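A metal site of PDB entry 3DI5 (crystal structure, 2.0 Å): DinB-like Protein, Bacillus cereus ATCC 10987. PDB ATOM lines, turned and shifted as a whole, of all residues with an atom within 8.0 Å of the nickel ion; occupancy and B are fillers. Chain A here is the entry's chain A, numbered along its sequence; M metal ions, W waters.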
ATOM      1  N   TRP A  41       5.107 -22.428   0.909  1.00  0.00           N
ATOM      2  CA  TRP A  41       4.901 -21.704  -0.341  1.00  0.00           C
ATOM      3  C   TRP A  41       5.357 -22.439  -1.591  1.00  0.00           C
ATOM      4  O   TRP A  41       6.306 -23.226  -1.550  1.00  0.00           O
ATOM      5  CB  TRP A  41       5.643 -20.372  -0.299  1.00  0.00           C
ATOM      6  CG  TRP A  41       4.913 -19.248   0.323  1.00  0.00           C
ATOM      7  CD1 TRP A  41       3.846 -19.318   1.185  1.00  0.00           C
ATOM      8  CD2 TRP A  41       5.217 -17.877   0.154  1.00  0.00           C
ATOM      9  NE1 TRP A  41       3.466 -18.040   1.561  1.00  0.00           N
ATOM     10  CE2 TRP A  41       4.295 -17.138   0.937  1.00  0.00           C
ATOM     11  CE3 TRP A  41       6.178 -17.174  -0.578  1.00  0.00           C
ATOM     12  CZ2 TRP A  41       4.311 -15.740   0.992  1.00  0.00           C
ATOM     13  CZ3 TRP A  41       6.203 -15.791  -0.509  1.00  0.00           C
ATOM     14  CH2 TRP A  41       5.269 -15.089   0.258  1.00  0.00           C
ATOM     15  N   VAL A  46       6.123 -17.363  -4.438  1.00  0.00           N
ATOM     16  CA  VAL A  46       7.384 -16.639  -4.408  1.00  0.00           C
ATOM     17  C   VAL A  46       7.460 -15.592  -5.524  1.00  0.00           C
ATOM     18  O   VAL A  46       7.792 -14.436  -5.247  1.00  0.00           O
ATOM     19  CB  VAL A  46       8.625 -17.587  -4.409  1.00  0.00           C
ATOM     20  CG1 VAL A  46       9.953 -16.759  -4.388  1.00  0.00           C
ATOM     21  CG2 VAL A  46       8.552 -18.510  -3.242  1.00  0.00           C
ATOM     22  N   HIS A  49       4.909 -12.714  -5.152  1.00  0.00           N
ATOM     23  CA  HIS A  49       5.311 -11.895  -4.019  1.00  0.00           C
ATOM     24  C   HIS A  49       6.344 -10.825  -4.466  1.00  0.00           C
ATOM     25  O   HIS A  49       6.295  -9.683  -4.022  1.00  0.00           O
ATOM     26  CB  HIS A  49       5.879 -12.812  -2.919  1.00  0.00           C
ATOM     27  CG  HIS A  49       6.353 -12.116  -1.684  1.00  0.00           C
ATOM     28  ND1 HIS A  49       5.498 -11.433  -0.842  1.00  0.00           N
ATOM     29  CD2 HIS A  49       7.569 -12.072  -1.092  1.00  0.00           C
ATOM     30  CE1 HIS A  49       6.184 -10.960   0.184  1.00  0.00           C
ATOM     31  NE2 HIS A  49       7.442 -11.328   0.058  1.00  0.00           N
ATOM     32  N   ILE A  50       7.233 -11.200  -5.387  1.00  0.00           N
ATOM     33  CA  ILE A  50       8.229 -10.282  -5.973  1.00  0.00           C
ATOM     34  C   ILE A  50       7.571  -9.186  -6.792  1.00  0.00           C
ATOM     35  O   ILE A  50       7.915  -7.985  -6.713  1.00  0.00           O
ATOM     36  CB  ILE A  50       9.207 -11.078  -6.888  1.00  0.00           C
ATOM     37  CG1 ILE A  50      10.185 -11.861  -6.009  1.00  0.00           C
ATOM     38  CG2 ILE A  50      10.030 -10.161  -7.867  1.00  0.00           C
ATOM     39  CD1 ILE A  50      10.806 -13.051  -6.696  1.00  0.00           C
ATOM     40  N   ALA A  53       5.612  -6.928  -4.332  1.00  0.00           N
ATOM     41  CA  ALA A  53       6.524  -6.231  -3.438  1.00  0.00           C
ATOM     42  C   ALA A  53       6.947  -4.848  -3.918  1.00  0.00           C
ATOM     43  O   ALA A  53       7.303  -4.014  -3.092  1.00  0.00           O
ATOM     44  CB  ALA A  53       7.778  -7.110  -3.118  1.00  0.00           C
ATOM     45  N   ILE A  57       6.579  -2.077  -0.978  1.00  0.00           N
ATOM     46  CA  ILE A  57       7.750  -1.458  -0.381  1.00  0.00           C
ATOM     47  C   ILE A  57       7.768   0.057  -0.707  1.00  0.00           C
ATOM     48  O   ILE A  57       8.116   0.872   0.147  1.00  0.00           O
ATOM     49  CB  ILE A  57       9.047  -2.199  -0.793  1.00  0.00           C
ATOM     50  CG1 ILE A  57       9.146  -3.546  -0.054  1.00  0.00           C
ATOM     51  CG2 ILE A  57      10.264  -1.318  -0.608  1.00  0.00           C
ATOM     52  CD1 ILE A  57      10.365  -4.409  -0.480  1.00  0.00           C
ATOM     53  N   ASP A  71      -0.621 -10.254  -2.609  1.00  0.00           N
ATOM     54  CA  ASP A  71       0.073 -11.443  -3.114  1.00  0.00           C
ATOM     55  C   ASP A  71      -0.740 -12.735  -2.990  1.00  0.00           C
ATOM     56  O   ASP A  71      -0.221 -13.822  -3.220  1.00  0.00           O
ATOM     57  CB  ASP A  71       1.518 -11.561  -2.524  1.00  0.00           C
ATOM     58  CG  ASP A  71       1.548 -11.979  -1.069  1.00  0.00           C
ATOM     59  OD1 ASP A  71       0.463 -12.119  -0.457  1.00  0.00           O
ATOM     60  OD2 ASP A  71       2.658 -12.163  -0.514  1.00  0.00           O
ATOM     61  N   HIS A 128      15.269  -7.231  -0.742  1.00  0.00           N
ATOM     62  CA  HIS A 128      14.093  -8.116  -0.613  1.00  0.00           C
ATOM     63  C   HIS A 128      13.953  -8.977  -1.859  1.00  0.00           C
ATOM     64  O   HIS A 128      13.854 -10.194  -1.746  1.00  0.00           O
ATOM     65  CB  HIS A 128      12.827  -7.263  -0.353  1.00  0.00           C
ATOM     66  CG  HIS A 128      11.545  -8.057  -0.307  1.00  0.00           C
ATOM     67  ND1 HIS A 128      10.626  -8.028  -1.341  1.00  0.00           N
ATOM     68  CD2 HIS A 128      11.023  -8.863   0.642  1.00  0.00           C
ATOM     69  CE1 HIS A 128       9.597  -8.800  -1.017  1.00  0.00           C
ATOM     70  NE2 HIS A 128       9.818  -9.316   0.180  1.00  0.00           N
ATOM     71  N   GLN A 129      13.926  -8.326  -3.028  1.00  0.00           N
ATOM     72  CA  GLN A 129      13.809  -8.993  -4.312  1.00  0.00           C
ATOM     73  C   GLN A 129      14.896 -10.039  -4.550  1.00  0.00           C
ATOM     74  O   GLN A 129      14.635 -11.094  -5.097  1.00  0.00           O
ATOM     75  CB  GLN A 129      13.870  -7.963  -5.407  1.00  0.00           C
ATOM     76  CG  GLN A 129      13.555  -8.527  -6.801  1.00  0.00           C
ATOM     77  CD  GLN A 129      13.542  -7.484  -7.844  1.00  0.00           C
ATOM     78  OE1 GLN A 129      12.503  -7.238  -8.478  1.00  0.00           O
ATOM     79  NE2 GLN A 129      14.696  -6.832  -8.055  1.00  0.00           N
ATOM     80  N   HIS A 131      16.755 -11.635  -2.197  1.00  0.00           N
ATOM     81  CA  HIS A 131      16.523 -12.760  -1.284  1.00  0.00           C
ATOM     82  C   HIS A 131      15.581 -13.804  -1.887  1.00  0.00           C
ATOM     83  O   HIS A 131      15.895 -14.997  -1.912  1.00  0.00           O
ATOM     84  CB  HIS A 131      15.932 -12.256   0.033  1.00  0.00           C
ATOM     85  CG  HIS A 131      15.319 -13.323   0.881  1.00  0.00           C
ATOM     86  ND1 HIS A 131      16.071 -14.255   1.552  1.00  0.00           N
ATOM     87  CD2 HIS A 131      14.027 -13.573   1.188  1.00  0.00           C
ATOM     88  CE1 HIS A 131      15.261 -15.050   2.236  1.00  0.00           C
ATOM     89  NE2 HIS A 131      14.015 -14.654   2.038  1.00  0.00           N
ATOM     90  N   HIS A 132      14.438 -13.328  -2.347  1.00  0.00           N
ATOM     91  CA  HIS A 132      13.388 -14.179  -2.918  1.00  0.00           C
ATOM     92  C   HIS A 132      13.712 -14.749  -4.287  1.00  0.00           C
ATOM     93  O   HIS A 132      13.297 -15.875  -4.632  1.00  0.00           O
ATOM     94  CB  HIS A 132      12.078 -13.405  -3.009  1.00  0.00           C
ATOM     95  CG  HIS A 132      11.374 -13.254  -1.697  1.00  0.00           C
ATOM     96  ND1 HIS A 132      10.887 -14.327  -0.997  1.00  0.00           N
ATOM     97  CD2 HIS A 132      11.079 -12.154  -0.964  1.00  0.00           C
ATOM     98  CE1 HIS A 132      10.306 -13.894   0.114  1.00  0.00           C
ATOM     99  NE2 HIS A 132      10.398 -12.585   0.144  1.00  0.00           N
ATOM    100  N   GLN A 135      15.636 -17.723  -3.678  1.00  0.00           N
ATOM    101  CA  GLN A 135      14.724 -18.839  -3.401  1.00  0.00           C
ATOM    102  C   GLN A 135      14.187 -19.405  -4.703  1.00  0.00           C
ATOM    103  O   GLN A 135      14.161 -20.615  -4.904  1.00  0.00           O
ATOM    104  CB  GLN A 135      13.544 -18.363  -2.553  1.00  0.00           C
ATOM    105  CG  GLN A 135      13.939 -17.856  -1.190  1.00  0.00           C
ATOM    106  CD  GLN A 135      12.743 -17.440  -0.294  1.00  0.00           C
ATOM    107  OE1 GLN A 135      11.763 -16.881  -0.758  1.00  0.00           O
ATOM    108  NE2 GLN A 135      12.876 -17.688   1.021  1.00  0.00           N
HETATM  109 NI    NI M   1       9.171 -11.119   1.562  1.00  0.00          NI
HETATM  110  O   HOH W   1       8.079 -12.872   2.797  1.00  0.00           O
HETATM  111  O   HOH W   2      10.692 -10.877   3.238  1.00  0.00           O
HETATM  112  O   HOH W   3       7.820  -9.594   2.754  1.00  0.00           O
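A ring nitrogen (ND1) of His 49 sits at hydrogen-bond distance from the side-chain carboxylate of Asp 71, 3.0 Å away. The side-chain amide oxygen (OE1) of Gln 135 sits at hydrogen-bond distance from a ring nitrogen (ND1) of His 132 (2.7 Å).
Of the 12 residues printed, 3 come within 4 Å of the nickel ion.
Water W2 binds the nickel ion. NE2 of His 49 is bound to the nickel ion (2.3 Å). The nickel ion is bound by water W3 (2.4 Å). NE2 of His 128 binds the nickel ion (2.4 Å). The nickel ion is bound by NE2 of His 132, 2.4 Å away. Water W1 binds the nickel ion, 2.4 Å away. The nickel ion has six donor atoms within binding distance.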
